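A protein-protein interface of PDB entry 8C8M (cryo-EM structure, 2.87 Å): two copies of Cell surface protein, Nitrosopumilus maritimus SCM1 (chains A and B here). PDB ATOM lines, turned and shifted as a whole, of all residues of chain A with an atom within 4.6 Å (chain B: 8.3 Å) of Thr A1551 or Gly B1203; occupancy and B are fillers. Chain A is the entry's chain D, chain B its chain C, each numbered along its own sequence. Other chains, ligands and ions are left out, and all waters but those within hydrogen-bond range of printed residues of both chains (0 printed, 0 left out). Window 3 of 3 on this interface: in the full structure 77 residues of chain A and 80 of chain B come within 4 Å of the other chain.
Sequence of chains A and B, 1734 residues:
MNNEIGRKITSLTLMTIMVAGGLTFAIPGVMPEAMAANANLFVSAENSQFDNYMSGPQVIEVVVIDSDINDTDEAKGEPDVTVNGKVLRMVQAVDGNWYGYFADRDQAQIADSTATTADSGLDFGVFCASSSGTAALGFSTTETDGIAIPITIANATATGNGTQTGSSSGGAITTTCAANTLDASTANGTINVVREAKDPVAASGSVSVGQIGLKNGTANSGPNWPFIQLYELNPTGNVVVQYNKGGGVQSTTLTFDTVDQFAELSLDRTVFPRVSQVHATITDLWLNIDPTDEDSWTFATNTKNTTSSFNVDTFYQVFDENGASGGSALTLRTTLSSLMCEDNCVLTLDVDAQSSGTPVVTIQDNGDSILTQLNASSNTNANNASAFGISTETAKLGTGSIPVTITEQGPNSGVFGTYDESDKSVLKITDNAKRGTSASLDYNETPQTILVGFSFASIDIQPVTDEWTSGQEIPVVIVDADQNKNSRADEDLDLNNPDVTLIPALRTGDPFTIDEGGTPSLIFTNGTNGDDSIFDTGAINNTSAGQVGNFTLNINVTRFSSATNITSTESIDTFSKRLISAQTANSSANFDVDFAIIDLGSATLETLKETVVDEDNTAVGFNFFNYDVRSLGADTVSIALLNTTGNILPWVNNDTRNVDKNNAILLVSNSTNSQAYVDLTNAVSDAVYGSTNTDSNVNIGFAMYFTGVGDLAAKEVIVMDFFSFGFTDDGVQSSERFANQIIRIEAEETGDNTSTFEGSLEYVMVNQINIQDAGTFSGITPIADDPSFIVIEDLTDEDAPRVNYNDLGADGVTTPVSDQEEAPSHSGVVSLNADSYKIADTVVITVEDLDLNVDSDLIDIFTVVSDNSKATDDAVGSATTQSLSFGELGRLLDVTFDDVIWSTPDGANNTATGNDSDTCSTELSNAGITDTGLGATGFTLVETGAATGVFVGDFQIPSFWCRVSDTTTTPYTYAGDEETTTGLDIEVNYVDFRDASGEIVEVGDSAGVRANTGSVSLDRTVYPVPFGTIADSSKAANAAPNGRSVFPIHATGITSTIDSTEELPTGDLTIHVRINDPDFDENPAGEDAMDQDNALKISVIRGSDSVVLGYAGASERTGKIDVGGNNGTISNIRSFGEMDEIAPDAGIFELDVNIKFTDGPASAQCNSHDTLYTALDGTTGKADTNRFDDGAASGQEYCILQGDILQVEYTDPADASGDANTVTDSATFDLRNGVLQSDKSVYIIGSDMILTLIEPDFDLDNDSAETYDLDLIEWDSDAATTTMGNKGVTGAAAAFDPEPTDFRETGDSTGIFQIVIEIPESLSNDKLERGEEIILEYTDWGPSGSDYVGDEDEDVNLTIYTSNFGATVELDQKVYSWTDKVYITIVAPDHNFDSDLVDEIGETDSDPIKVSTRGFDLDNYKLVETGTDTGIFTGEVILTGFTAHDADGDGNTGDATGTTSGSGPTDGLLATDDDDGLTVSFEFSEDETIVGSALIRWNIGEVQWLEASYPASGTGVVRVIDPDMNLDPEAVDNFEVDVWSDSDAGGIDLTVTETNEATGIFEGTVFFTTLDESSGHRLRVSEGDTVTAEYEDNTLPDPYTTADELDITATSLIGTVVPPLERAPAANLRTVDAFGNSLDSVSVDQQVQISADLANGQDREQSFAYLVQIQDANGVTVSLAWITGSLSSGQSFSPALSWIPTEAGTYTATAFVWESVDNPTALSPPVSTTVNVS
O of Gly B1203 sits at hydrogen-bond distance from ND2 of Asn A1534.
N of Gly B1103 lies within hydrogen-bond range of OD1 of Asn A1534 (3.1 Å).
OE1 of Gln B1202 lies within hydrogen-bond range of NE2 of His A1577.
The side-chain carboxylate of Asp B1230 sits at hydrogen-bond distance from the side-chain amide nitrogen of Gln B1202 (3.3 Å).
N of Leu B1201 is in hydrogen-bond range of OD2 of Asp B1204, at 3.0 Å.
The backbone carbonyl oxygen of Asp B1204 lies within hydrogen-bond range of the backbone NH of Phe B1229 (3.0 Å).
N of Ile B1101 lies within hydrogen-bond range of O of Ile B1205.
O of Thr B1228 is in hydrogen-bond range of N of Tyr B1023 (2.9 Å).
OD2 of Asp B1204 lies within salt-bridge range of NH1 of Arg B1102, at 2.4 Å.
Asn A1534 touches Ile B1101 (ND2 to O, 3.5 Å).
Arg B1102 touches Asn A1534 (CA to ND2, 3.8 Å).
Asn A1534 touches Asp B1204 (ND2 to CA, 3.5 Å).
Asn A1534 touches Ile B1205.
Thr A1551 touches Gln B1202 (OG1 to O, 3.9 Å).
CG2 of Thr A1551 touches O of Gly B1203 (3.3 Å).
Gly B1203 touches Thr A1553 (O to CG2, 3.7 Å).
CG2 of Thr A1553 touches CD1 of Ile B1205, 3.5 Å away.
CG2 of Thr B1228 touches CG2 of Thr A1553, 3.7 Å away.
His A1577 touches Asp B1347.
Thr A1551 touches just these residues of chain B: Gln B1202 and Gly B1203.
Printed residues of chain A within 4 Å of Asp B1204: Asn A1534 (3.5 Å).
Printed residues of chain A within 4 Å of Thr B1228: Thr A1553.
Printed residues of chain A within 4 Å of Arg B1102: Asn A1534 (3.8 Å).
Of the printed residues of chain B, His A1577 touches Gln B1202 and Asp B1347.
Printed residues of chain A within 4 Å of Ile B1101: Asn A1534 (3.5 Å).
The nearest printed residue of chain A that does not touch Gly B1203 is Val A1552 (5.2 Å).
Hydrophobic or aromatic side chains of chain B within 4 Å of the printed part of chain A: Ile B1205.
Hydrophobic or aromatic side chains of chain A within 4 Å of the printed part of chain B: His A1577.
Among the printed residues, no Asp or Glu carboxylate lies within 4 Å of a Lys or Arg side-chain nitrogen of the other chain.
No position is printed for both chains.
Of the 13 pairs that touch across the chains among the printed residues, none has its exchanged pair printed and touching as well.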
ATOM      1  N   ASN A1534      21.392 -30.408  21.878  1.00  0.00           N
ATOM      2  CA  ASN A1534      21.008 -30.628  20.464  1.00  0.00           C
ATOM      3  C   ASN A1534      21.609 -31.940  19.964  1.00  0.00           C
ATOM      4  O   ASN A1534      22.764 -32.249  20.309  1.00  0.00           O
ATOM      5  CB  ASN A1534      21.443 -29.461  19.580  1.00  0.00           C
ATOM      6  CG  ASN A1534      22.939 -29.183  19.622  1.00  0.00           C
ATOM      7  OD1 ASN A1534      23.641 -29.632  20.527  1.00  0.00           O
ATOM      8  ND2 ASN A1534      23.454 -28.474  18.627  1.00  0.00           N
ATOM      9  N   PHE A1535      20.857 -32.669  19.151  1.00  0.00           N
ATOM     10  CA  PHE A1535      21.347 -33.892  18.471  1.00  0.00           C
ATOM     11  C   PHE A1535      20.630 -34.026  17.128  1.00  0.00           C
ATOM     12  O   PHE A1535      19.562 -33.410  16.926  1.00  0.00           O
ATOM     13  CB  PHE A1535      21.173 -35.102  19.391  1.00  0.00           C
ATOM     14  CG  PHE A1535      19.748 -35.554  19.580  1.00  0.00           C
ATOM     15  CD1 PHE A1535      19.062 -35.277  20.757  1.00  0.00           C
ATOM     16  CD2 PHE A1535      19.100 -36.271  18.584  1.00  0.00           C
ATOM     17  CE1 PHE A1535      17.757 -35.710  20.930  1.00  0.00           C
ATOM     18  CE2 PHE A1535      17.789 -36.695  18.761  1.00  0.00           C
ATOM     19  CZ  PHE A1535      17.124 -36.425  19.938  1.00  0.00           C
ATOM     20  N   GLU A1536      21.187 -34.848  16.241  1.00  0.00           N
ATOM     21  CA  GLU A1536      20.769 -34.904  14.817  1.00  0.00           C
ATOM     22  C   GLU A1536      19.846 -36.099  14.599  1.00  0.00           C
ATOM     23  O   GLU A1536      20.270 -37.242  14.823  1.00  0.00           O
ATOM     24  CB  GLU A1536      21.975 -34.971  13.892  1.00  0.00           C
ATOM     25  CG  GLU A1536      23.027 -33.926  14.221  1.00  0.00           C
ATOM     26  CD  GLU A1536      24.229 -33.881  13.288  1.00  0.00           C
ATOM     27  OE1 GLU A1536      24.090 -34.278  12.111  1.00  0.00           O
ATOM     28  OE2 GLU A1536      25.311 -33.446  13.744  1.00  0.00           O
ATOM     29  N   ASP A1549      19.895 -34.561   7.602  1.00  0.00           N
ATOM     30  CA  ASP A1549      20.089 -34.744   9.063  1.00  0.00           C
ATOM     31  C   ASP A1549      19.472 -33.544   9.793  1.00  0.00           C
ATOM     32  O   ASP A1549      20.056 -32.441   9.758  1.00  0.00           O
ATOM     33  CB  ASP A1549      21.558 -35.000   9.403  1.00  0.00           C
ATOM     34  CG  ASP A1549      22.579 -34.023   8.828  1.00  0.00           C
ATOM     35  OD1 ASP A1549      22.182 -32.930   8.367  1.00  0.00           O
ATOM     36  OD2 ASP A1549      23.778 -34.364   8.846  1.00  0.00           O
ATOM     37  N   LEU A1550      18.319 -33.752  10.432  1.00  0.00           N
ATOM     38  CA  LEU A1550      17.592 -32.695  11.181  1.00  0.00           C
ATOM     39  C   LEU A1550      18.236 -32.542  12.559  1.00  0.00           C
ATOM     40  O   LEU A1550      18.269 -33.517  13.326  1.00  0.00           O
ATOM     41  CB  LEU A1550      16.115 -33.084  11.288  1.00  0.00           C
ATOM     42  CG  LEU A1550      15.137 -31.945  11.575  1.00  0.00           C
ATOM     43  CD1 LEU A1550      13.695 -32.385  11.367  1.00  0.00           C
ATOM     44  CD2 LEU A1550      15.316 -31.398  12.981  1.00  0.00           C
ATOM     45  N   THR A1551      18.743 -31.353  12.851  1.00  0.00           N
ATOM     46  CA  THR A1551      19.235 -30.963  14.191  1.00  0.00           C
ATOM     47  C   THR A1551      18.052 -30.515  15.047  1.00  0.00           C
ATOM     48  O   THR A1551      17.533 -29.411  14.824  1.00  0.00           O
ATOM     49  CB  THR A1551      20.309 -29.881  14.083  1.00  0.00           C
ATOM     50  OG1 THR A1551      21.263 -30.304  13.109  1.00  0.00           O
ATOM     51  CG2 THR A1551      20.984 -29.641  15.416  1.00  0.00           C
ATOM     52  N   VAL A1552      17.659 -31.341  16.008  1.00  0.00           N
ATOM     53  CA  VAL A1552      16.594 -30.988  16.989  1.00  0.00           C
ATOM     54  C   VAL A1552      17.268 -30.355  18.203  1.00  0.00           C
ATOM     55  O   VAL A1552      18.451 -30.653  18.465  1.00  0.00           O
ATOM     56  CB  VAL A1552      15.733 -32.196  17.384  1.00  0.00           C
ATOM     57  CG1 VAL A1552      14.827 -32.624  16.245  1.00  0.00           C
ATOM     58  CG2 VAL A1552      16.589 -33.359  17.861  1.00  0.00           C
ATOM     59  N   THR A1553      16.540 -29.493  18.903  1.00  0.00           N
ATOM     60  CA  THR A1553      17.070 -28.763  20.080  1.00  0.00           C
ATOM     61  C   THR A1553      16.083 -28.842  21.235  1.00  0.00           C
ATOM     62  O   THR A1553      14.877 -28.953  21.007  1.00  0.00           O
ATOM     63  CB  THR A1553      17.416 -27.309  19.751  1.00  0.00           C
ATOM     64  OG1 THR A1553      16.217 -26.627  19.378  1.00  0.00           O
ATOM     65  CG2 THR A1553      18.458 -27.197  18.660  1.00  0.00           C
ATOM     66  N   GLU A1563      12.958 -30.398  19.346  1.00  0.00           N
ATOM     67  CA  GLU A1563      12.174 -29.991  18.153  1.00  0.00           C
ATOM     68  C   GLU A1563      13.111 -29.383  17.117  1.00  0.00           C
ATOM     69  O   GLU A1563      14.140 -28.818  17.505  1.00  0.00           O
ATOM     70  CB  GLU A1563      11.073 -29.009  18.545  1.00  0.00           C
ATOM     71  CG  GLU A1563      10.009 -29.636  19.435  1.00  0.00           C
ATOM     72  CD  GLU A1563       8.863 -28.739  19.882  1.00  0.00           C
ATOM     73  OE1 GLU A1563       8.627 -27.689  19.235  1.00  0.00           O
ATOM     74  OE2 GLU A1563       8.210 -29.091  20.893  1.00  0.00           O
ATOM     75  N   GLY A1564      12.750 -29.493  15.842  1.00  0.00           N
ATOM     76  CA  GLY A1564      13.539 -28.924  14.733  1.00  0.00           C
ATOM     77  C   GLY A1564      12.671 -28.569  13.544  1.00  0.00           C
ATOM     78  O   GLY A1564      11.480 -28.903  13.554  1.00  0.00           O
ATOM     79  N   HIS A1577      18.331 -28.216   5.794  1.00  0.00           N
ATOM     80  CA  HIS A1577      17.005 -28.562   6.378  1.00  0.00           C
ATOM     81  C   HIS A1577      15.932 -28.487   5.291  1.00  0.00           C
ATOM     82  O   HIS A1577      14.777 -28.321   5.643  1.00  0.00           O
ATOM     83  CB  HIS A1577      16.747 -27.725   7.641  1.00  0.00           C
ATOM     84  CG  HIS A1577      17.521 -28.231   8.816  1.00  0.00           C
ATOM     85  ND1 HIS A1577      16.957 -28.489  10.005  1.00  0.00           N
ATOM     86  CD2 HIS A1577      18.819 -28.639   8.954  1.00  0.00           C
ATOM     87  CE1 HIS A1577      17.846 -28.919  10.863  1.00  0.00           C
ATOM     88  NE2 HIS A1577      18.991 -29.051  10.234  1.00  0.00           N
ATOM     89  N   TYR B1023      19.441 -17.269  16.926  1.00  0.00           N
ATOM     90  CA  TYR B1023      20.449 -16.391  16.298  1.00  0.00           C
ATOM     91  C   TYR B1023      20.673 -16.783  14.844  1.00  0.00           C
ATOM     92  O   TYR B1023      20.614 -17.957  14.478  1.00  0.00           O
ATOM     93  CB  TYR B1023      21.746 -16.445  17.088  1.00  0.00           C
ATOM     94  CG  TYR B1023      21.702 -15.669  18.371  1.00  0.00           C
ATOM     95  CD1 TYR B1023      21.316 -16.268  19.556  1.00  0.00           C
ATOM     96  CD2 TYR B1023      22.058 -14.336  18.396  1.00  0.00           C
ATOM     97  CE1 TYR B1023      21.283 -15.559  20.745  1.00  0.00           C
ATOM     98  CE2 TYR B1023      22.031 -13.608  19.575  1.00  0.00           C
ATOM     99  CZ  TYR B1023      21.648 -14.228  20.752  1.00  0.00           C
ATOM    100  OH  TYR B1023      21.629 -13.562  21.933  1.00  0.00           O
ATOM    101  N   VAL B1025      23.116 -17.579  11.695  1.00  0.00           N
ATOM    102  CA  VAL B1025      24.475 -18.139  11.504  1.00  0.00           C
ATOM    103  C   VAL B1025      25.339 -17.060  10.865  1.00  0.00           C
ATOM    104  O   VAL B1025      25.011 -16.563   9.790  1.00  0.00           O
ATOM    105  CB  VAL B1025      24.429 -19.406  10.644  1.00  0.00           C
ATOM    106  CG1 VAL B1025      25.824 -19.937  10.413  1.00  0.00           C
ATOM    107  CG2 VAL B1025      23.541 -20.464  11.270  1.00  0.00           C
ATOM    108  N   VAL B1100      30.085 -23.060  22.693  1.00  0.00           N
ATOM    109  CA  VAL B1100      29.255 -23.562  21.569  1.00  0.00           C
ATOM    110  C   VAL B1100      29.380 -25.083  21.530  1.00  0.00           C
ATOM    111  O   VAL B1100      30.514 -25.594  21.479  1.00  0.00           O
ATOM    112  CB  VAL B1100      29.653 -22.908  20.238  1.00  0.00           C
ATOM    113  CG1 VAL B1100      28.962 -23.574  19.057  1.00  0.00           C
ATOM    114  CG2 VAL B1100      29.343 -21.422  20.256  1.00  0.00           C
ATOM    115  N   ILE B1101      28.240 -25.766  21.540  1.00  0.00           N
ATOM    116  CA  ILE B1101      28.182 -27.254  21.578  1.00  0.00           C
ATOM    117  C   ILE B1101      27.394 -27.740  20.360  1.00  0.00           C
ATOM    118  O   ILE B1101      26.398 -27.095  19.988  1.00  0.00           O
ATOM    119  CB  ILE B1101      27.590 -27.737  22.916  1.00  0.00           C
ATOM    120  CG1 ILE B1101      26.069 -27.572  22.971  1.00  0.00           C
ATOM    121  CG2 ILE B1101      28.262 -27.031  24.091  1.00  0.00           C
ATOM    122  CD1 ILE B1101      25.452 -28.080  24.248  1.00  0.00           C
ATOM    123  N   ARG B1102      27.845 -28.838  19.764  1.00  0.00           N
ATOM    124  CA  ARG B1102      27.125 -29.543  18.677  1.00  0.00           C
ATOM    125  C   ARG B1102      27.076 -31.025  19.041  1.00  0.00           C
ATOM    126  O   ARG B1102      28.123 -31.699  18.941  1.00  0.00           O
ATOM    127  CB  ARG B1102      27.811 -29.312  17.330  1.00  0.00           C
ATOM    128  CG  ARG B1102      27.214 -30.144  16.203  1.00  0.00           C
ATOM    129  CD  ARG B1102      27.566 -29.660  14.811  1.00  0.00           C
ATOM    130  NE  ARG B1102      28.976 -29.298  14.673  1.00  0.00           N
ATOM    131  CZ  ARG B1102      29.448 -28.079  14.403  1.00  0.00           C
ATOM    132  NH1 ARG B1102      28.633 -27.053  14.214  1.00  0.00           N
ATOM    133  NH2 ARG B1102      30.754 -27.892  14.300  1.00  0.00           N
ATOM    134  N   GLY B1103      25.900 -31.504  19.449  1.00  0.00           N
ATOM    135  CA  GLY B1103      25.732 -32.862  19.996  1.00  0.00           C
ATOM    136  C   GLY B1103      26.599 -33.055  21.227  1.00  0.00           C
ATOM    137  O   GLY B1103      26.410 -32.323  22.216  1.00  0.00           O
ATOM    138  N   ILE B1200      30.584 -22.996  12.599  1.00  0.00           N
ATOM    139  CA  ILE B1200      29.195 -23.034  13.126  1.00  0.00           C
ATOM    140  C   ILE B1200      28.293 -23.553  12.017  1.00  0.00           C
ATOM    141  O   ILE B1200      28.400 -23.078  10.873  1.00  0.00           O
ATOM    142  CB  ILE B1200      28.714 -21.658  13.608  1.00  0.00           C
ATOM    143  CG1 ILE B1200      29.583 -21.113  14.738  1.00  0.00           C
ATOM    144  CG2 ILE B1200      27.246 -21.716  13.999  1.00  0.00           C
ATOM    145  CD1 ILE B1200      30.768 -20.343  14.246  1.00  0.00           C
ATOM    146  N   LEU B1201      27.421 -24.485  12.370  1.00  0.00           N
ATOM    147  CA  LEU B1201      26.383 -25.004  11.453  1.00  0.00           C
ATOM    148  C   LEU B1201      25.027 -24.527  11.969  1.00  0.00           C
ATOM    149  O   LEU B1201      24.945 -24.039  13.104  1.00  0.00           O
ATOM    150  CB  LEU B1201      26.459 -26.536  11.370  1.00  0.00           C
ATOM    151  CG  LEU B1201      27.447 -27.141  10.364  1.00  0.00           C
ATOM    152  CD1 LEU B1201      27.219 -26.639   8.946  1.00  0.00           C
ATOM    153  CD2 LEU B1201      28.881 -26.881  10.756  1.00  0.00           C
ATOM    154  N   GLN B1202      23.994 -24.681  11.147  1.00  0.00           N
ATOM    155  CA  GLN B1202      22.588 -24.509  11.586  1.00  0.00           C
ATOM    156  C   GLN B1202      22.265 -25.586  12.630  1.00  0.00           C
ATOM    157  O   GLN B1202      22.656 -26.758  12.439  1.00  0.00           O
ATOM    158  CB  GLN B1202      21.645 -24.553  10.384  1.00  0.00           C
ATOM    159  CG  GLN B1202      20.217 -24.149  10.727  1.00  0.00           C
ATOM    160  CD  GLN B1202      19.378 -25.276  11.280  1.00  0.00           C
ATOM    161  OE1 GLN B1202      19.583 -26.439  10.947  1.00  0.00           O
ATOM    162  NE2 GLN B1202      18.416 -24.945  12.126  1.00  0.00           N
ATOM    163  N   GLY B1203      21.551 -25.196  13.683  1.00  0.00           N
ATOM    164  CA  GLY B1203      21.075 -26.102  14.747  1.00  0.00           C
ATOM    165  C   GLY B1203      22.041 -26.198  15.917  1.00  0.00           C
ATOM    166  O   GLY B1203      21.670 -26.847  16.929  1.00  0.00           O
ATOM    167  N   ASP B1204      23.195 -25.531  15.851  1.00  0.00           N
ATOM    168  CA  ASP B1204      24.167 -25.504  16.975  1.00  0.00           C
ATOM    169  C   ASP B1204      23.560 -24.802  18.198  1.00  0.00           C
ATOM    170  O   ASP B1204      22.504 -24.145  18.090  1.00  0.00           O
ATOM    171  CB  ASP B1204      25.482 -24.840  16.576  1.00  0.00           C
ATOM    172  CG  ASP B1204      26.193 -25.539  15.436  1.00  0.00           C
ATOM    173  OD1 ASP B1204      25.548 -26.362  14.737  1.00  0.00           O
ATOM    174  OD2 ASP B1204      27.386 -25.245  15.241  1.00  0.00           O
ATOM    175  N   ILE B1205      24.217 -24.960  19.339  1.00  0.00           N
ATOM    176  CA  ILE B1205      23.715 -24.449  20.641  1.00  0.00           C
ATOM    177  C   ILE B1205      24.739 -23.493  21.246  1.00  0.00           C
ATOM    178  O   ILE B1205      25.930 -23.829  21.318  1.00  0.00           O
ATOM    179  CB  ILE B1205      23.379 -25.615  21.580  1.00  0.00           C
ATOM    180  CG1 ILE B1205      22.341 -26.546  20.951  1.00  0.00           C
ATOM    181  CG2 ILE B1205      22.933 -25.095  22.936  1.00  0.00           C
ATOM    182  CD1 ILE B1205      21.016 -25.914  20.648  1.00  0.00           C
ATOM    183  N   LEU B1206      24.252 -22.338  21.691  1.00  0.00           N
ATOM    184  CA  LEU B1206      25.033 -21.354  22.472  1.00  0.00           C
ATOM    185  C   LEU B1206      24.501 -21.339  23.904  1.00  0.00           C
ATOM    186  O   LEU B1206      23.295 -21.067  24.092  1.00  0.00           O
ATOM    187  CB  LEU B1206      24.883 -19.987  21.809  1.00  0.00           C
ATOM    188  CG  LEU B1206      25.791 -18.878  22.334  1.00  0.00           C
ATOM    189  CD1 LEU B1206      27.251 -19.316  22.419  1.00  0.00           C
ATOM    190  CD2 LEU B1206      25.640 -17.661  21.442  1.00  0.00           C
ATOM    191  N   ALA B1227      20.684 -20.899  23.763  1.00  0.00           N
ATOM    192  CA  ALA B1227      20.073 -20.437  22.503  1.00  0.00           C
ATOM    193  C   ALA B1227      20.597 -21.271  21.336  1.00  0.00           C
ATOM    194  O   ALA B1227      21.614 -21.971  21.482  1.00  0.00           O
ATOM    195  CB  ALA B1227      20.375 -18.975  22.308  1.00  0.00           C
ATOM    196  N   THR B1228      19.923 -21.170  20.195  1.00  0.00           N
ATOM    197  CA  THR B1228      20.225 -21.989  18.998  1.00  0.00           C
ATOM    198  C   THR B1228      20.597 -21.082  17.833  1.00  0.00           C
ATOM    199  O   THR B1228      19.991 -20.003  17.706  1.00  0.00           O
ATOM    200  CB  THR B1228      19.029 -22.868  18.624  1.00  0.00           C
ATOM    201  OG1 THR B1228      17.975 -22.052  18.108  1.00  0.00           O
ATOM    202  CG2 THR B1228      18.507 -23.655  19.805  1.00  0.00           C
ATOM    203  N   PHE B1229      21.487 -21.560  16.970  1.00  0.00           N
ATOM    204  CA  PHE B1229      21.753 -20.926  15.656  1.00  0.00           C
ATOM    205  C   PHE B1229      20.755 -21.473  14.645  1.00  0.00           C
ATOM    206  O   PHE B1229      20.379 -22.650  14.726  1.00  0.00           O
ATOM    207  CB  PHE B1229      23.185 -21.158  15.192  1.00  0.00           C
ATOM    208  CG  PHE B1229      24.219 -20.473  16.045  1.00  0.00           C
ATOM    209  CD1 PHE B1229      24.559 -20.976  17.291  1.00  0.00           C
ATOM    210  CD2 PHE B1229      24.877 -19.340  15.587  1.00  0.00           C
ATOM    211  CE1 PHE B1229      25.531 -20.358  18.063  1.00  0.00           C
ATOM    212  CE2 PHE B1229      25.854 -18.729  16.360  1.00  0.00           C
ATOM    213  CZ  PHE B1229      26.178 -19.234  17.597  1.00  0.00           C
ATOM    214  N   ASP B1230      20.320 -20.625  13.725  1.00  0.00           N
ATOM    215  CA  ASP B1230      19.303 -21.016  12.724  1.00  0.00           C
ATOM    216  C   ASP B1230      19.427 -20.106  11.506  1.00  0.00           C
ATOM    217  O   ASP B1230      19.906 -18.983  11.660  1.00  0.00           O
ATOM    218  CB  ASP B1230      17.914 -21.022  13.362  1.00  0.00           C
ATOM    219  CG  ASP B1230      16.830 -21.586  12.461  1.00  0.00           C
ATOM    220  OD1 ASP B1230      17.164 -22.017  11.332  1.00  0.00           O
ATOM    221  OD2 ASP B1230      15.662 -21.613  12.905  1.00  0.00           O
ATOM    222  N   LEU B1231      18.998 -20.599  10.344  1.00  0.00           N
ATOM    223  CA  LEU B1231      18.856 -19.800   9.099  1.00  0.00           C
ATOM    224  C   LEU B1231      17.426 -19.927   8.574  1.00  0.00           C
ATOM    225  O   LEU B1231      16.810 -21.003   8.689  1.00  0.00           O
ATOM    226  CB  LEU B1231      19.877 -20.256   8.052  1.00  0.00           C
ATOM    227  CG  LEU B1231      21.346 -19.967   8.378  1.00  0.00           C
ATOM    228  CD1 LEU B1231      22.274 -20.718   7.428  1.00  0.00           C
ATOM    229  CD2 LEU B1231      21.643 -18.470   8.343  1.00  0.00           C
ATOM    230  N   SER B1346      20.196 -24.382   3.285  1.00  0.00           N
ATOM    231  CA  SER B1346      21.660 -24.364   3.517  1.00  0.00           C
ATOM    232  C   SER B1346      21.967 -24.681   4.986  1.00  0.00           C
ATOM    233  O   SER B1346      21.137 -24.397   5.868  1.00  0.00           O
ATOM    234  CB  SER B1346      22.267 -23.075   3.075  1.00  0.00           C
ATOM    235  OG  SER B1346      23.648 -23.073   3.384  1.00  0.00           O
ATOM    236  N   ASP B1347      23.138 -25.255   5.224  1.00  0.00           N
ATOM    237  CA  ASP B1347      23.642 -25.542   6.590  1.00  0.00           C
ATOM    238  C   ASP B1347      24.524 -24.396   7.077  1.00  0.00           C
ATOM    239  O   ASP B1347      24.513 -24.135   8.289  1.00  0.00           O
ATOM    240  CB  ASP B1347      24.371 -26.882   6.620  1.00  0.00           C
ATOM    241  CG  ASP B1347      23.423 -28.056   6.757  1.00  0.00           C
ATOM    242  OD1 ASP B1347      23.863 -29.203   6.510  1.00  0.00           O
ATOM    243  OD2 ASP B1347      22.250 -27.816   7.122  1.00  0.00           O
